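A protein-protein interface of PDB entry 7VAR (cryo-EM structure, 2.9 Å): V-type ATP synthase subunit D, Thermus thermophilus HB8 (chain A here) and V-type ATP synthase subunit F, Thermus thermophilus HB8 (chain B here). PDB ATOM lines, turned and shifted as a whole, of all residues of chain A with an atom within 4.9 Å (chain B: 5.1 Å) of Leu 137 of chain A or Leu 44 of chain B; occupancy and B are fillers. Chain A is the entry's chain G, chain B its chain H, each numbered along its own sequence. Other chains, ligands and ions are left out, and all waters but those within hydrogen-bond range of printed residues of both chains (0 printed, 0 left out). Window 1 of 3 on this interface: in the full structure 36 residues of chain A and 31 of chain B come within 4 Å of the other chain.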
ATOM      1  N   LEU A  53     -21.503   0.126   1.683  1.00  0.00           N
ATOM      2  CA  LEU A  53     -21.510  -1.138   0.954  1.00  0.00           C
ATOM      3  C   LEU A  53     -22.458  -2.143   1.595  1.00  0.00           C
ATOM      4  O   LEU A  53     -23.132  -2.902   0.892  1.00  0.00           O
ATOM      5  CB  LEU A  53     -20.097  -1.713   0.879  1.00  0.00           C
ATOM      6  CG  LEU A  53     -19.960  -3.061   0.168  1.00  0.00           C
ATOM      7  CD1 LEU A  53     -20.385  -2.949  -1.284  1.00  0.00           C
ATOM      8  CD2 LEU A  53     -18.537  -3.574   0.269  1.00  0.00           C
ATOM      9  N   LEU A 104      -8.999   1.670  -8.450  1.00  0.00           N
ATOM     10  CA  LEU A 104      -9.899   0.941  -9.330  1.00  0.00           C
ATOM     11  C   LEU A 104     -11.163   1.742  -9.615  1.00  0.00           C
ATOM     12  O   LEU A 104     -11.754   2.345  -8.715  1.00  0.00           O
ATOM     13  CB  LEU A 104     -10.275  -0.405  -8.711  1.00  0.00           C
ATOM     14  CG  LEU A 104      -9.130  -1.367  -8.391  1.00  0.00           C
ATOM     15  CD1 LEU A 104      -9.676  -2.739  -8.029  1.00  0.00           C
ATOM     16  CD2 LEU A 104      -8.167  -1.464  -9.561  1.00  0.00           C
ATOM     17  N   TYR A 133     -24.426  -1.991  -5.996  1.00  0.00           N
ATOM     18  CA  TYR A 133     -23.621  -2.772  -5.065  1.00  0.00           C
ATOM     19  C   TYR A 133     -22.159  -2.814  -5.499  1.00  0.00           C
ATOM     20  O   TYR A 133     -21.250  -2.593  -4.690  1.00  0.00           O
ATOM     21  CB  TYR A 133     -24.218  -4.176  -4.969  1.00  0.00           C
ATOM     22  CG  TYR A 133     -23.446  -5.165  -4.142  1.00  0.00           C
ATOM     23  CD1 TYR A 133     -23.269  -4.981  -2.781  1.00  0.00           C
ATOM     24  CD2 TYR A 133     -22.923  -6.309  -4.724  1.00  0.00           C
ATOM     25  CE1 TYR A 133     -22.569  -5.900  -2.028  1.00  0.00           C
ATOM     26  CE2 TYR A 133     -22.227  -7.230  -3.981  1.00  0.00           C
ATOM     27  CZ  TYR A 133     -22.053  -7.024  -2.635  1.00  0.00           C
ATOM     28  OH  TYR A 133     -21.358  -7.950  -1.900  1.00  0.00           O
ATOM     29  N   ALA A 134     -21.915  -3.082  -6.783  1.00  0.00           N
ATOM     30  CA  ALA A 134     -20.546  -3.066  -7.294  1.00  0.00           C
ATOM     31  C   ALA A 134     -19.939  -1.667  -7.231  1.00  0.00           C
ATOM     32  O   ALA A 134     -18.729  -1.518  -6.995  1.00  0.00           O
ATOM     33  CB  ALA A 134     -20.512  -3.597  -8.726  1.00  0.00           C
ATOM     34  N   GLU A 135     -20.759  -0.637  -7.452  1.00  0.00           N
ATOM     35  CA  GLU A 135     -20.279   0.738  -7.354  1.00  0.00           C
ATOM     36  C   GLU A 135     -19.789   1.053  -5.946  1.00  0.00           C
ATOM     37  O   GLU A 135     -18.779   1.744  -5.772  1.00  0.00           O
ATOM     38  CB  GLU A 135     -21.388   1.707  -7.769  1.00  0.00           C
ATOM     39  CG  GLU A 135     -20.994   3.175  -7.708  1.00  0.00           C
ATOM     40  CD  GLU A 135     -19.910   3.534  -8.706  1.00  0.00           C
ATOM     41  OE1 GLU A 135     -19.816   2.862  -9.756  1.00  0.00           O
ATOM     42  OE2 GLU A 135     -19.148   4.487  -8.441  1.00  0.00           O
ATOM     43  N   ALA A 136     -20.505   0.576  -4.927  1.00  0.00           N
ATOM     44  CA  ALA A 136     -20.012   0.730  -3.560  1.00  0.00           C
ATOM     45  C   ALA A 136     -18.790  -0.148  -3.301  1.00  0.00           C
ATOM     46  O   ALA A 136     -17.880   0.247  -2.551  1.00  0.00           O
ATOM     47  CB  ALA A 136     -21.122   0.408  -2.561  1.00  0.00           C
ATOM     48  N   LEU A 137     -18.755  -1.336  -3.910  1.00  0.00           N
ATOM     49  CA  LEU A 137     -17.654  -2.267  -3.691  1.00  0.00           C
ATOM     50  C   LEU A 137     -16.327  -1.690  -4.168  1.00  0.00           C
ATOM     51  O   LEU A 137     -15.296  -1.863  -3.506  1.00  0.00           O
ATOM     52  CB  LEU A 137     -17.947  -3.590  -4.399  1.00  0.00           C
ATOM     53  CG  LEU A 137     -16.996  -4.758  -4.138  1.00  0.00           C
ATOM     54  CD1 LEU A 137     -17.072  -5.200  -2.686  1.00  0.00           C
ATOM     55  CD2 LEU A 137     -17.311  -5.917  -5.070  1.00  0.00           C
ATOM     56  N   ILE A 138     -16.326  -1.014  -5.319  1.00  0.00           N
ATOM     57  CA  ILE A 138     -15.065  -0.463  -5.817  1.00  0.00           C
ATOM     58  C   ILE A 138     -14.551   0.643  -4.895  1.00  0.00           C
ATOM     59  O   ILE A 138     -13.340   0.748  -4.652  1.00  0.00           O
ATOM     60  CB  ILE A 138     -15.206   0.024  -7.272  1.00  0.00           C
ATOM     61  CG1 ILE A 138     -16.258   1.125  -7.392  1.00  0.00           C
ATOM     62  CG2 ILE A 138     -15.543  -1.142  -8.192  1.00  0.00           C
ATOM     63  CD1 ILE A 138     -16.281   1.803  -8.743  1.00  0.00           C
ATOM     64  N   ARG A 139     -15.451   1.471  -4.358  1.00  0.00           N
ATOM     65  CA  ARG A 139     -15.053   2.494  -3.394  1.00  0.00           C
ATOM     66  C   ARG A 139     -14.444   1.865  -2.147  1.00  0.00           C
ATOM     67  O   ARG A 139     -13.414   2.330  -1.633  1.00  0.00           O
ATOM     68  CB  ARG A 139     -16.265   3.351  -3.029  1.00  0.00           C
ATOM     69  CG  ARG A 139     -16.015   4.384  -1.946  1.00  0.00           C
ATOM     70  CD  ARG A 139     -17.329   4.975  -1.460  1.00  0.00           C
ATOM     71  NE  ARG A 139     -17.186   5.692  -0.198  1.00  0.00           N
ATOM     72  CZ  ARG A 139     -18.201   6.074   0.564  1.00  0.00           C
ATOM     73  NH1 ARG A 139     -19.454   5.827   0.220  1.00  0.00           N
ATOM     74  NH2 ARG A 139     -17.953   6.721   1.700  1.00  0.00           N
ATOM     75  N   VAL A 140     -15.077   0.804  -1.642  1.00  0.00           N
ATOM     76  CA  VAL A 140     -14.557   0.129  -0.456  1.00  0.00           C
ATOM     77  C   VAL A 140     -13.171  -0.441  -0.737  1.00  0.00           C
ATOM     78  O   VAL A 140     -12.254  -0.336   0.086  1.00  0.00           O
ATOM     79  CB  VAL A 140     -15.535  -0.961   0.015  1.00  0.00           C
ATOM     80  CG1 VAL A 140     -14.870  -1.873   1.031  1.00  0.00           C
ATOM     81  CG2 VAL A 140     -16.779  -0.326   0.600  1.00  0.00           C
ATOM     82  N   ALA A 141     -12.999  -1.050  -1.912  1.00  0.00           N
ATOM     83  CA  ALA A 141     -11.695  -1.598  -2.273  1.00  0.00           C
ATOM     84  C   ALA A 141     -10.634  -0.506  -2.329  1.00  0.00           C
ATOM     85  O   ALA A 141      -9.512  -0.694  -1.841  1.00  0.00           O
ATOM     86  CB  ALA A 141     -11.785  -2.328  -3.612  1.00  0.00           C
ATOM     87  N   MET B   1     -15.126  -7.758 -11.834  1.00  0.00           N
ATOM     88  CA  MET B   1     -14.892  -8.929 -12.671  1.00  0.00           C
ATOM     89  C   MET B   1     -15.520 -10.183 -12.075  1.00  0.00           C
ATOM     90  O   MET B   1     -16.636 -10.555 -12.434  1.00  0.00           O
ATOM     91  CB  MET B   1     -13.392  -9.147 -12.881  1.00  0.00           C
ATOM     92  CG  MET B   1     -12.736  -8.120 -13.788  1.00  0.00           C
ATOM     93  SD  MET B   1     -13.537  -8.002 -15.396  1.00  0.00           S
ATOM     94  CE  MET B   1     -13.000  -9.530 -16.159  1.00  0.00           C
ATOM     95  N   ALA B   2     -14.805 -10.829 -11.158  1.00  0.00           N
ATOM     96  CA  ALA B   2     -15.227 -12.099 -10.590  1.00  0.00           C
ATOM     97  C   ALA B   2     -15.409 -11.978  -9.084  1.00  0.00           C
ATOM     98  O   ALA B   2     -14.614 -11.331  -8.395  1.00  0.00           O
ATOM     99  CB  ALA B   2     -14.216 -13.208 -10.899  1.00  0.00           C
ATOM    100  N   VAL B   3     -16.469 -12.606  -8.581  1.00  0.00           N
ATOM    101  CA  VAL B   3     -16.749 -12.675  -7.151  1.00  0.00           C
ATOM    102  C   VAL B   3     -17.140 -14.106  -6.811  1.00  0.00           C
ATOM    103  O   VAL B   3     -17.873 -14.755  -7.565  1.00  0.00           O
ATOM    104  CB  VAL B   3     -17.864 -11.695  -6.727  1.00  0.00           C
ATOM    105  CG1 VAL B   3     -18.081 -11.761  -5.223  1.00  0.00           C
ATOM    106  CG2 VAL B   3     -17.530 -10.274  -7.156  1.00  0.00           C
ATOM    107  N   TYR B  42      -8.925  -9.817 -13.970  1.00  0.00           N
ATOM    108  CA  TYR B  42      -8.534  -8.423 -13.820  1.00  0.00           C
ATOM    109  C   TYR B  42      -8.968  -7.859 -12.473  1.00  0.00           C
ATOM    110  O   TYR B  42     -10.120  -8.008 -12.058  1.00  0.00           O
ATOM    111  CB  TYR B  42      -9.129  -7.579 -14.948  1.00  0.00           C
ATOM    112  CG  TYR B  42      -8.770  -8.056 -16.336  1.00  0.00           C
ATOM    113  CD1 TYR B  42      -7.447  -8.106 -16.754  1.00  0.00           C
ATOM    114  CD2 TYR B  42      -9.755  -8.441 -17.235  1.00  0.00           C
ATOM    115  CE1 TYR B  42      -7.114  -8.536 -18.023  1.00  0.00           C
ATOM    116  CE2 TYR B  42      -9.433  -8.873 -18.508  1.00  0.00           C
ATOM    117  CZ  TYR B  42      -8.110  -8.918 -18.897  1.00  0.00           C
ATOM    118  OH  TYR B  42      -7.782  -9.347 -20.163  1.00  0.00           O
ATOM    119  N   ALA B  43      -8.024  -7.210 -11.792  1.00  0.00           N
ATOM    120  CA  ALA B  43      -8.294  -6.362 -10.637  1.00  0.00           C
ATOM    121  C   ALA B  43      -9.092  -7.053  -9.536  1.00  0.00           C
ATOM    122  O   ALA B  43      -8.642  -8.048  -8.959  1.00  0.00           O
ATOM    123  CB  ALA B  43      -9.027  -5.095 -11.082  1.00  0.00           C
ATOM    124  N   LEU B  44     -10.282  -6.530  -9.253  1.00  0.00           N
ATOM    125  CA  LEU B  44     -11.015  -6.911  -8.054  1.00  0.00           C
ATOM    126  C   LEU B  44     -11.551  -8.332  -8.168  1.00  0.00           C
ATOM    127  O   LEU B  44     -12.162  -8.701  -9.175  1.00  0.00           O
ATOM    128  CB  LEU B  44     -12.159  -5.926  -7.811  1.00  0.00           C
ATOM    129  CG  LEU B  44     -12.950  -5.987  -6.501  1.00  0.00           C
ATOM    130  CD1 LEU B  44     -13.489  -4.607  -6.167  1.00  0.00           C
ATOM    131  CD2 LEU B  44     -14.096  -6.984  -6.577  1.00  0.00           C
ATOM    132  N   VAL B  45     -11.315  -9.131  -7.128  1.00  0.00           N
ATOM    133  CA  VAL B  45     -11.903 -10.458  -6.985  1.00  0.00           C
ATOM    134  C   VAL B  45     -12.449 -10.538  -5.564  1.00  0.00           C
ATOM    135  O   VAL B  45     -11.716 -10.884  -4.631  1.00  0.00           O
ATOM    136  CB  VAL B  45     -10.899 -11.584  -7.254  1.00  0.00           C
ATOM    137  CG1 VAL B  45     -11.587 -12.937  -7.160  1.00  0.00           C
ATOM    138  CG2 VAL B  45     -10.245 -11.410  -8.617  1.00  0.00           C
ATOM    139  N   ALA B  46     -13.729 -10.222  -5.394  1.00  0.00           N
ATOM    140  CA  ALA B  46     -14.338 -10.256  -4.073  1.00  0.00           C
ATOM    141  C   ALA B  46     -14.634 -11.690  -3.653  1.00  0.00           C
ATOM    142  O   ALA B  46     -14.893 -12.564  -4.484  1.00  0.00           O
ATOM    143  CB  ALA B  46     -15.621  -9.425  -4.049  1.00  0.00           C
ATOM    144  N   PRO B  69      -4.364  -7.175  -8.839  1.00  0.00           N
ATOM    145  CA  PRO B  69      -5.573  -7.674  -8.168  1.00  0.00           C
ATOM    146  C   PRO B  69      -5.787  -7.027  -6.808  1.00  0.00           C
ATOM    147  O   PRO B  69      -4.837  -6.702  -6.092  1.00  0.00           O
ATOM    148  CB  PRO B  69      -5.310  -9.178  -8.035  1.00  0.00           C
ATOM    149  CG  PRO B  69      -3.840  -9.295  -8.014  1.00  0.00           C
ATOM    150  CD  PRO B  69      -3.347  -8.238  -8.955  1.00  0.00           C
ATOM    151  N   VAL B  70      -7.059  -6.848  -6.458  1.00  0.00           N
ATOM    152  CA  VAL B  70      -7.475  -6.305  -5.166  1.00  0.00           C
ATOM    153  C   VAL B  70      -8.528  -7.255  -4.612  1.00  0.00           C
ATOM    154  O   VAL B  70      -9.605  -7.409  -5.198  1.00  0.00           O
ATOM    155  CB  VAL B  70      -8.025  -4.880  -5.276  1.00  0.00           C
ATOM    156  CG1 VAL B  70      -8.459  -4.381  -3.909  1.00  0.00           C
ATOM    157  CG2 VAL B  70      -6.982  -3.951  -5.875  1.00  0.00           C
ATOM    158  N   LEU B  72     -10.871  -8.456  -1.248  1.00  0.00           N
ATOM    159  CA  LEU B  72     -11.446  -7.984   0.001  1.00  0.00           C
ATOM    160  C   LEU B  72     -12.582  -8.909   0.406  1.00  0.00           C
ATOM    161  O   LEU B  72     -13.206  -9.537  -0.459  1.00  0.00           O
ATOM    162  CB  LEU B  72     -11.959  -6.540  -0.128  1.00  0.00           C
ATOM    163  CG  LEU B  72     -13.288  -6.303  -0.850  1.00  0.00           C
ATOM    164  CD1 LEU B  72     -13.811  -4.918  -0.534  1.00  0.00           C
ATOM    165  CD2 LEU B  72     -13.145  -6.480  -2.355  1.00  0.00           C
ATOM    166  N   ILE B  74     -16.410  -9.789   1.897  1.00  0.00           N
ATOM    167  CA  ILE B  74     -17.735  -9.184   1.832  1.00  0.00           C
ATOM    168  C   ILE B  74     -18.764 -10.234   2.230  1.00  0.00           C
ATOM    169  O   ILE B  74     -18.592 -11.427   1.972  1.00  0.00           O
ATOM    170  CB  ILE B  74     -18.023  -8.602   0.427  1.00  0.00           C
ATOM    171  CG1 ILE B  74     -19.367  -7.875   0.408  1.00  0.00           C
ATOM    172  CG2 ILE B  74     -17.980  -9.697  -0.632  1.00  0.00           C
ATOM    173  CD1 ILE B  74     -19.519  -6.831   1.493  1.00  0.00           C
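N of Val 70 of chain B is in hydrogen-bond range of O of Ala 43 of chain B (3.2 Å). O of Val 70 of chain B lies within hydrogen-bond range of N of Val 45 of chain B (3.1 Å).
Ile 74 of chain B touches Leu 53 of chain A. Ala 43 of chain B touches Leu 104 of chain A (CB to CD1, 3.9 Å). Val 70 of chain B touches Leu 104 of chain A. CG1 of Ile 74 of chain B touches OH of Tyr 133 of chain A, 3.0 Å away. Leu 137 of chain A touches Leu 44 of chain B. Leu 72 of chain B touches Leu 137 of chain A (CD1 to CD1, 3.9 Å). Leu 72 of chain B touches Val 140 of chain A. CB of Ala 141 of chain A touches CD1 of Leu 44 of chain B, at 3.8 Å. Ala 141 of chain A touches Val 70 of chain B (CB to CG1, 3.9 Å).
Leu 44 of chain B touches two residues of chain A. Of the printed residues of chain A, Val 70 of chain B touches Leu 104 (3.7 Å) and Ala 141 (3.9 Å). Of the printed residues of chain A, Leu 72 of chain B touches Leu 137 and Val 140.
Of the 12 printed residues of chain B, 5 touch a printed residue of chain A. Printed residues of chain B that touch a printed residue of chain A: Ala 43, Leu 44, Val 70, Leu 72 and Ile 74. Hydrophobic or aromatic side chains of chain B that line the printed part of chain A: Ala 43, Leu 44, Val 70, Leu 72 and Ile 74. Printed residues of chain A that touch a printed residue of chain B: Leu 53, Leu 104, Tyr 133, Leu 137, Val 140 and Ala 141. Hydrophobic or aromatic side chains of chain A that line the printed part of chain B: Leu 53, Leu 104, Tyr 133, Leu 137, Val 140 and Ala 141. Among the printed residues, 9 pairs touch across the chains.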
